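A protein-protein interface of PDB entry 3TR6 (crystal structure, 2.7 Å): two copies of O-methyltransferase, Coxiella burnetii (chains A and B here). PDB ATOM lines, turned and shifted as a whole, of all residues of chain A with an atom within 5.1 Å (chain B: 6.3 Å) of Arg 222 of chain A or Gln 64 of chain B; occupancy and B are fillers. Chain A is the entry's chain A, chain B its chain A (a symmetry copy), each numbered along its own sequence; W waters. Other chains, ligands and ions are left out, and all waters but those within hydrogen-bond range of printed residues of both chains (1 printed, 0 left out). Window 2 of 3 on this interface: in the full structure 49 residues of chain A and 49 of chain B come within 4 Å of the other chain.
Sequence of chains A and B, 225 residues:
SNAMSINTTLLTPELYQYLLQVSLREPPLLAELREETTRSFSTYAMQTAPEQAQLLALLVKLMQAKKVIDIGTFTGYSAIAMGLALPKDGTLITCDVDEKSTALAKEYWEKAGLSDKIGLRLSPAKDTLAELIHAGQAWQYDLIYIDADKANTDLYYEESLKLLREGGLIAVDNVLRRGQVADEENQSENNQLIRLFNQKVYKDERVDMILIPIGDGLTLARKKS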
ATOM      1  N   GLY A 167      35.520  21.600 -17.183  1.00  0.00           N
ATOM      2  CA  GLY A 167      34.135  21.886 -17.505  1.00  0.00           C
ATOM      3  C   GLY A 167      33.843  21.783 -18.992  1.00  0.00           C
ATOM      4  O   GLY A 167      32.745  22.111 -19.436  1.00  0.00           O
ATOM      5  N   GLY A 168      34.827  21.331 -19.765  1.00  0.00           N
ATOM      6  CA  GLY A 168      34.642  21.103 -21.186  1.00  0.00           C
ATOM      7  C   GLY A 168      33.707  19.934 -21.435  1.00  0.00           C
ATOM      8  O   GLY A 168      33.427  19.152 -20.522  1.00  0.00           O
ATOM      9  N   LEU A 169      33.229  19.803 -22.669  1.00  0.00           N
ATOM     10  CA  LEU A 169      32.222  18.791 -22.979  1.00  0.00           C
ATOM     11  C   LEU A 169      32.584  17.870 -24.146  1.00  0.00           C
ATOM     12  O   LEU A 169      32.935  18.333 -25.232  1.00  0.00           O
ATOM     13  CB  LEU A 169      30.872  19.456 -23.251  1.00  0.00           C
ATOM     14  CG  LEU A 169      29.703  18.498 -23.465  1.00  0.00           C
ATOM     15  CD1 LEU A 169      29.379  17.761 -22.169  1.00  0.00           C
ATOM     16  CD2 LEU A 169      28.476  19.232 -23.993  1.00  0.00           C
ATOM     17  N   ILE A 170      32.490  16.565 -23.909  1.00  0.00           N
ATOM     18  CA  ILE A 170      32.590  15.575 -24.977  1.00  0.00           C
ATOM     19  C   ILE A 170      31.197  15.111 -25.390  1.00  0.00           C
ATOM     20  O   ILE A 170      30.390  14.731 -24.546  1.00  0.00           O
ATOM     21  CB  ILE A 170      33.376  14.327 -24.540  1.00  0.00           C
ATOM     22  CG1 ILE A 170      34.827  14.680 -24.224  1.00  0.00           C
ATOM     23  CG2 ILE A 170      33.325  13.267 -25.626  1.00  0.00           C
ATOM     24  CD1 ILE A 170      35.599  13.546 -23.610  1.00  0.00           C
ATOM     25  N   ARG A 206      36.050  10.837 -13.934  1.00  0.00           N
ATOM     26  CA  ARG A 206      36.674  12.067 -14.397  1.00  0.00           C
ATOM     27  C   ARG A 206      35.642  12.995 -15.026  1.00  0.00           C
ATOM     28  O   ARG A 206      35.931  14.156 -15.328  1.00  0.00           O
ATOM     29  CB  ARG A 206      37.758  11.745 -15.419  1.00  0.00           C
ATOM     30  CG  ARG A 206      38.843  10.832 -14.895  1.00  0.00           C
ATOM     31  CD  ARG A 206      39.790  10.424 -15.998  1.00  0.00           C
ATOM     32  NE  ARG A 206      39.153   9.523 -16.950  1.00  0.00           N
ATOM     33  CZ  ARG A 206      39.767   8.992 -17.998  1.00  0.00           C
ATOM     34  NH1 ARG A 206      41.041   9.273 -18.231  1.00  0.00           N
ATOM     35  NH2 ARG A 206      39.107   8.181 -18.815  1.00  0.00           N
ATOM     36  N   VAL A 207      34.433  12.473 -15.218  1.00  0.00           N
ATOM     37  CA  VAL A 207      33.382  13.207 -15.911  1.00  0.00           C
ATOM     38  C   VAL A 207      32.029  13.081 -15.224  1.00  0.00           C
ATOM     39  O   VAL A 207      31.802  12.166 -14.436  1.00  0.00           O
ATOM     40  CB  VAL A 207      33.213  12.706 -17.361  1.00  0.00           C
ATOM     41  CG1 VAL A 207      34.487  12.905 -18.151  1.00  0.00           C
ATOM     42  CG2 VAL A 207      32.804  11.237 -17.366  1.00  0.00           C
ATOM     43  N   ASP A 208      31.143  14.023 -15.525  1.00  0.00           N
ATOM     44  CA  ASP A 208      29.718  13.864 -15.271  1.00  0.00           C
ATOM     45  C   ASP A 208      29.081  13.627 -16.630  1.00  0.00           C
ATOM     46  O   ASP A 208      29.440  14.283 -17.607  1.00  0.00           O
ATOM     47  CB  ASP A 208      29.126  15.116 -14.619  1.00  0.00           C
ATOM     48  CG  ASP A 208      29.572  15.293 -13.178  1.00  0.00           C
ATOM     49  OD1 ASP A 208      29.608  14.287 -12.438  1.00  0.00           O
ATOM     50  OD2 ASP A 208      29.897  16.436 -12.790  1.00  0.00           O
ATOM     51  N   MET A 209      28.149  12.688 -16.709  1.00  0.00           N
ATOM     52  CA  MET A 209      27.627  12.302 -18.015  1.00  0.00           C
ATOM     53  C   MET A 209      26.121  12.088 -18.079  1.00  0.00           C
ATOM     54  O   MET A 209      25.417  12.124 -17.067  1.00  0.00           O
ATOM     55  CB  MET A 209      28.374  11.073 -18.551  1.00  0.00           C
ATOM     56  CG  MET A 209      28.331   9.849 -17.643  1.00  0.00           C
ATOM     57  SD  MET A 209      26.708   8.786 -17.870  1.00  0.00           S
ATOM     58  CE  MET A 209      27.014   8.106 -19.673  1.00  0.00           C
ATOM     59  N   LEU A 220      26.892  12.674 -23.412  1.00  0.00           N
ATOM     60  CA  LEU A 220      27.582  13.903 -23.052  1.00  0.00           C
ATOM     61  C   LEU A 220      28.411  13.659 -21.800  1.00  0.00           C
ATOM     62  O   LEU A 220      27.909  13.132 -20.813  1.00  0.00           O
ATOM     63  CB  LEU A 220      26.588  15.033 -22.811  1.00  0.00           C
ATOM     64  CG  LEU A 220      25.590  15.272 -23.940  1.00  0.00           C
ATOM     65  CD1 LEU A 220      24.605  16.372 -23.568  1.00  0.00           C
ATOM     66  CD2 LEU A 220      26.310  15.604 -25.238  1.00  0.00           C
ATOM     67  N   ALA A 221      29.684  14.033 -21.853  1.00  0.00           N
ATOM     68  CA  ALA A 221      30.582  13.870 -20.717  1.00  0.00           C
ATOM     69  C   ALA A 221      31.300  15.182 -20.409  1.00  0.00           C
ATOM     70  O   ALA A 221      32.141  15.639 -21.184  1.00  0.00           O
ATOM     71  CB  ALA A 221      31.581  12.760 -20.985  1.00  0.00           C
ATOM     72  N   ARG A 222      30.951  15.786 -19.277  1.00  0.00           N
ATOM     73  CA  ARG A 222      31.593  17.015 -18.831  1.00  0.00           C
ATOM     74  C   ARG A 222      32.825  16.713 -17.978  1.00  0.00           C
ATOM     75  O   ARG A 222      32.739  15.998 -16.980  1.00  0.00           O
ATOM     76  CB  ARG A 222      30.603  17.869 -18.039  1.00  0.00           C
ATOM     77  CG  ARG A 222      31.173  19.178 -17.536  1.00  0.00           C
ATOM     78  CD  ARG A 222      30.201  19.883 -16.606  1.00  0.00           C
ATOM     79  NE  ARG A 222      30.766  21.129 -16.103  1.00  0.00           N
ATOM     80  CZ  ARG A 222      31.520  21.219 -15.014  1.00  0.00           C
ATOM     81  NH1 ARG A 222      31.794  20.132 -14.304  1.00  0.00           N
ATOM     82  NH2 ARG A 222      31.998  22.396 -14.635  1.00  0.00           N
ATOM     83  N   LYS A 223      33.967  17.261 -18.377  1.00  0.00           N
ATOM     84  CA  LYS A 223      35.213  17.072 -17.643  1.00  0.00           C
ATOM     85  C   LYS A 223      35.164  17.790 -16.291  1.00  0.00           C
ATOM     86  O   LYS A 223      35.074  19.018 -16.232  1.00  0.00           O
ATOM     87  CB  LYS A 223      36.396  17.578 -18.475  1.00  0.00           C
ATOM     88  CG  LYS A 223      37.756  17.277 -17.870  1.00  0.00           C
ATOM     89  CD  LYS A 223      38.881  17.797 -18.752  1.00  0.00           C
ATOM     90  CE  LYS A 223      40.245  17.459 -18.167  1.00  0.00           C
ATOM     91  NZ  LYS A 223      41.354  18.054 -18.962  1.00  0.00           N
ATOM     92  N   LYS A 224      35.225  17.013 -15.211  1.00  0.00           N
ATOM     93  CA  LYS A 224      35.109  17.549 -13.857  1.00  0.00           C
ATOM     94  C   LYS A 224      36.312  18.375 -13.416  1.00  0.00           C
ATOM     95  O   LYS A 224      37.411  18.254 -13.969  1.00  0.00           O
ATOM     96  CB  LYS A 224      34.850  16.429 -12.843  1.00  0.00           C
ATOM     97  CG  LYS A 224      33.533  15.717 -13.043  1.00  0.00           C
ATOM     98  CD  LYS A 224      33.008  15.113 -11.753  1.00  0.00           C
ATOM     99  CE  LYS A 224      33.891  13.986 -11.257  1.00  0.00           C
ATOM    100  NZ  LYS A 224      33.161  13.100 -10.301  1.00  0.00           N
ATOM    101  N   SER A 225      36.089  19.208 -12.400  1.00  0.00           N
ATOM    102  CA  SER A 225      37.143  20.046 -11.823  1.00  0.00           C
ATOM    103  C   SER A 225      38.209  19.200 -11.119  1.00  0.00           C
ATOM    104  O   SER A 225      37.917  18.111 -10.619  1.00  0.00           O
ATOM    105  CB  SER A 225      36.537  21.050 -10.833  1.00  0.00           C
ATOM    106  OG  SER A 225      35.329  21.617 -11.341  1.00  0.00           O
ATOM    107  OXT SER A 225      39.383  19.574 -11.034  1.00  0.00           O
ATOM    108  N   LEU B  58      23.334  18.192 -14.962  1.00  0.00           N
ATOM    109  CA  LEU B  58      24.420  18.402 -15.909  1.00  0.00           C
ATOM    110  C   LEU B  58      24.369  19.810 -16.499  1.00  0.00           C
ATOM    111  O   LEU B  58      25.406  20.424 -16.737  1.00  0.00           O
ATOM    112  CB  LEU B  58      24.388  17.352 -17.024  1.00  0.00           C
ATOM    113  CG  LEU B  58      25.609  17.315 -17.956  1.00  0.00           C
ATOM    114  CD1 LEU B  58      26.858  16.840 -17.220  1.00  0.00           C
ATOM    115  CD2 LEU B  58      25.345  16.432 -19.162  1.00  0.00           C
ATOM    116  N   LEU B  59      23.161  20.320 -16.721  1.00  0.00           N
ATOM    117  CA  LEU B  59      22.986  21.662 -17.266  1.00  0.00           C
ATOM    118  C   LEU B  59      23.437  22.744 -16.290  1.00  0.00           C
ATOM    119  O   LEU B  59      24.041  23.739 -16.692  1.00  0.00           O
ATOM    120  CB  LEU B  59      21.528  21.892 -17.664  1.00  0.00           C
ATOM    121  CG  LEU B  59      21.033  21.062 -18.847  1.00  0.00           C
ATOM    122  CD1 LEU B  59      19.560  21.330 -19.105  1.00  0.00           C
ATOM    123  CD2 LEU B  59      21.860  21.355 -20.079  1.00  0.00           C
ATOM    124  N   VAL B  60      23.136  22.552 -15.011  1.00  0.00           N
ATOM    125  CA  VAL B  60      23.599  23.464 -13.973  1.00  0.00           C
ATOM    126  C   VAL B  60      25.125  23.558 -13.993  1.00  0.00           C
ATOM    127  O   VAL B  60      25.696  24.642 -13.873  1.00  0.00           O
ATOM    128  CB  VAL B  60      23.128  23.018 -12.569  1.00  0.00           C
ATOM    129  CG1 VAL B  60      23.883  23.776 -11.480  1.00  0.00           C
ATOM    130  CG2 VAL B  60      21.627  23.212 -12.419  1.00  0.00           C
ATOM    131  N   LYS B  61      25.783  22.416 -14.156  1.00  0.00           N
ATOM    132  CA  LYS B  61      27.239  22.383 -14.178  1.00  0.00           C
ATOM    133  C   LYS B  61      27.825  23.025 -15.437  1.00  0.00           C
ATOM    134  O   LYS B  61      28.813  23.757 -15.363  1.00  0.00           O
ATOM    135  CB  LYS B  61      27.748  20.948 -14.010  1.00  0.00           C
ATOM    136  CG  LYS B  61      27.545  20.388 -12.607  1.00  0.00           C
ATOM    137  CD  LYS B  61      28.004  18.942 -12.514  1.00  0.00           C
ATOM    138  CE  LYS B  61      28.580  18.626 -11.137  1.00  0.00           C
ATOM    139  NZ  LYS B  61      27.638  17.842 -10.290  1.00  0.00           N
ATOM    140  N   LEU B  62      27.215  22.761 -16.589  1.00  0.00           N
ATOM    141  CA  LEU B  62      27.710  23.310 -17.848  1.00  0.00           C
ATOM    142  C   LEU B  62      27.603  24.830 -17.883  1.00  0.00           C
ATOM    143  O   LEU B  62      28.506  25.519 -18.359  1.00  0.00           O
ATOM    144  CB  LEU B  62      26.966  22.702 -19.037  1.00  0.00           C
ATOM    145  CG  LEU B  62      27.413  21.309 -19.478  1.00  0.00           C
ATOM    146  CD1 LEU B  62      26.431  20.733 -20.481  1.00  0.00           C
ATOM    147  CD2 LEU B  62      28.816  21.354 -20.057  1.00  0.00           C
ATOM    148  N   MET B  63      26.493  25.351 -17.374  1.00  0.00           N
ATOM    149  CA  MET B  63      26.277  26.789 -17.361  1.00  0.00           C
ATOM    150  C   MET B  63      26.948  27.421 -16.161  1.00  0.00           C
ATOM    151  O   MET B  63      27.102  28.639 -16.101  1.00  0.00           O
ATOM    152  CB  MET B  63      24.787  27.107 -17.324  1.00  0.00           C
ATOM    153  CG  MET B  63      24.008  26.467 -18.439  1.00  0.00           C
ATOM    154  SD  MET B  63      22.126  26.889 -18.300  1.00  0.00           S
ATOM    155  CE  MET B  63      22.183  28.781 -18.779  1.00  0.00           C
ATOM    156  N   GLN B  64      27.354  26.586 -15.210  1.00  0.00           N
ATOM    157  CA  GLN B  64      27.811  27.081 -13.924  1.00  0.00           C
ATOM    158  C   GLN B  64      26.740  28.019 -13.382  1.00  0.00           C
ATOM    159  O   GLN B  64      27.011  29.174 -13.051  1.00  0.00           O
ATOM    160  CB  GLN B  64      29.143  27.812 -14.069  1.00  0.00           C
ATOM    161  CG  GLN B  64      30.184  27.374 -13.068  1.00  0.00           C
ATOM    162  CD  GLN B  64      30.598  25.938 -13.272  1.00  0.00           C
ATOM    163  OE1 GLN B  64      31.242  25.605 -14.266  1.00  0.00           O
ATOM    164  NE2 GLN B  64      30.220  25.074 -12.340  1.00  0.00           N
ATOM    165  N   ALA B  65      25.514  27.514 -13.320  1.00  0.00           N
ATOM    166  CA  ALA B  65      24.372  28.307 -12.896  1.00  0.00           C
ATOM    167  C   ALA B  65      24.482  28.663 -11.419  1.00  0.00           C
ATOM    168  O   ALA B  65      24.653  27.788 -10.571  1.00  0.00           O
ATOM    169  CB  ALA B  65      23.082  27.557 -13.174  1.00  0.00           C
ATOM    170  N   LYS B  66      24.386  29.954 -11.115  1.00  0.00           N
ATOM    171  CA  LYS B  66      24.523  30.429  -9.741  1.00  0.00           C
ATOM    172  C   LYS B  66      23.180  30.856  -9.156  1.00  0.00           C
ATOM    173  O   LYS B  66      23.055  31.064  -7.951  1.00  0.00           O
ATOM    174  CB  LYS B  66      25.533  31.575  -9.668  1.00  0.00           C
ATOM    175  CG  LYS B  66      26.928  31.189 -10.143  1.00  0.00           C
ATOM    176  CD  LYS B  66      27.865  32.385 -10.159  1.00  0.00           C
ATOM    177  CE  LYS B  66      29.202  32.043 -10.804  1.00  0.00           C
ATOM    178  NZ  LYS B  66      29.930  30.976 -10.064  1.00  0.00           N
ATOM    179  N   LYS B  67      22.179  30.978 -10.021  1.00  0.00           N
ATOM    180  CA  LYS B  67      20.834  31.355  -9.603  1.00  0.00           C
ATOM    181  C   LYS B  67      19.783  30.534 -10.343  1.00  0.00           C
ATOM    182  O   LYS B  67      19.542  30.743 -11.535  1.00  0.00           O
ATOM    183  CB  LYS B  67      20.594  32.845  -9.845  1.00  0.00           C
ATOM    184  CG  LYS B  67      21.124  33.757  -8.757  1.00  0.00           C
ATOM    185  CD  LYS B  67      20.537  35.146  -8.928  1.00  0.00           C
ATOM    186  CE  LYS B  67      20.569  35.943  -7.637  1.00  0.00           C
ATOM    187  NZ  LYS B  67      19.708  37.157  -7.736  1.00  0.00           N
ATOM    188  N   ALA B  85      24.264  20.095  -7.773  1.00  0.00           N
ATOM    189  CA  ALA B  85      25.156  20.448  -8.872  1.00  0.00           C
ATOM    190  C   ALA B  85      25.594  21.908  -8.803  1.00  0.00           C
ATOM    191  O   ALA B  85      26.530  22.318  -9.492  1.00  0.00           O
ATOM    192  CB  ALA B  85      24.492  20.151 -10.211  1.00  0.00           C
ATOM    193  N   LEU B  86      24.914  22.683  -7.963  1.00  0.00           N
ATOM    194  CA  LEU B  86      25.220  24.097  -7.778  1.00  0.00           C
ATOM    195  C   LEU B  86      26.674  24.329  -7.400  1.00  0.00           C
ATOM    196  O   LEU B  86      27.233  23.595  -6.586  1.00  0.00           O
ATOM    197  CB  LEU B  86      24.328  24.693  -6.691  1.00  0.00           C
ATOM    198  CG  LEU B  86      22.894  25.080  -7.049  1.00  0.00           C
ATOM    199  CD1 LEU B  86      22.137  25.476  -5.790  1.00  0.00           C
ATOM    200  CD2 LEU B  86      22.873  26.208  -8.073  1.00  0.00           C
ATOM    201  N   PRO B  87      27.293  25.358  -7.996  1.00  0.00           N
ATOM    202  CA  PRO B  87      28.630  25.778  -7.564  1.00  0.00           C
ATOM    203  C   PRO B  87      28.568  26.358  -6.152  1.00  0.00           C
ATOM    204  O   PRO B  87      27.470  26.635  -5.665  1.00  0.00           O
ATOM    205  CB  PRO B  87      29.013  26.851  -8.589  1.00  0.00           C
ATOM    206  CG  PRO B  87      27.725  27.309  -9.178  1.00  0.00           C
ATOM    207  CD  PRO B  87      26.816  26.125  -9.158  1.00  0.00           C
ATOM    208  N   ASP B 142      19.731  32.193 -14.109  1.00  0.00           N
ATOM    209  CA  ASP B 142      20.466  31.421 -15.101  1.00  0.00           C
ATOM    210  C   ASP B 142      19.632  30.278 -15.664  1.00  0.00           C
ATOM    211  O   ASP B 142      19.652  30.013 -16.865  1.00  0.00           O
ATOM    212  CB  ASP B 142      21.740  30.866 -14.470  1.00  0.00           C
ATOM    213  CG  ASP B 142      22.657  31.960 -13.968  1.00  0.00           C
ATOM    214  OD1 ASP B 142      22.871  32.946 -14.711  1.00  0.00           O
ATOM    215  OD2 ASP B 142      23.151  31.840 -12.828  1.00  0.00           O
HETATM  216  O   HOH W   1      30.965  23.506 -18.138  1.00  0.00           O
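O of Lys 61 of chain B sits at hydrogen-bond distance from NE of Arg 222 of chain A (3.4 Å).
The guanidinium group (NH2) of Arg 222 of chain A is in hydrogen-bond range of the side-chain amide oxygen (OE1) of Gln 64 of chain B (3.3 Å).
OD2 of Asp 208 of chain A lies within salt-bridge range of NZ of Lys 61 of chain B.
O of Lys 61 of chain B lies close to OE1 of Gln 64 of chain B (3.2 Å).
The backbone NH (N) of Arg 222 of chain A is in hydrogen-bond range of the backbone carbonyl oxygen (O) of Asp 208 of chain A (2.7 Å).
O of Asp 208 of chain A touches CD1 of Leu 58 of chain B, at 3.7 Å.
Leu 58 of chain B touches Arg 222 of chain A (CD1 to CB, 3.97 Å).
Leu 62 of chain B touches Arg 222 of chain A (N to NE, 3.9 Å).
Of the printed residues of chain B, Asp 208 of chain A touches Leu 58 (3.7 Å) and Lys 61 (3.0 Å).
Of the printed residues of chain B, Arg 222 of chain A touches Leu 58, Lys 61, Leu 62 and Gln 64.
Of the printed residues of chain A, Leu 58 of chain B touches Asp 208 and Arg 222.
Of the printed residues of chain A, Lys 61 of chain B touches Asp 208 (3.0 Å) and Arg 222 (3.4 Å).
Printed residues of chain A within 4 Å of Leu 62 of chain B: Arg 222.
Of chain A, only Arg 222 (3.3 Å) comes within 4 Å of Gln 64 of chain B.
The nearest residue of chain B that does not touch Arg 222 of chain A is Met 63 of chain B (6.1 Å).
The nearest printed residue of chain A that does not touch Leu 62 of chain B is Gly 167 of chain A (4.05 Å).
Printed residues of chain B that touch a printed residue of chain A: Leu 58, Lys 61, Leu 62 and Gln 64.
Among the printed residues, 6 pairs touch across the chains.
No position is printed for both chains.
Of the 6 pairs that touch across the chains among the printed residues, none has its exchanged pair printed and touching as well.
Water W1 lies within hydrogen-bond range of O of Gly 167 of chain A (2.6 Å), NE of Arg 222 of chain A (3.1 Å) and O of Leu 62 of chain B (3.2 Å).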
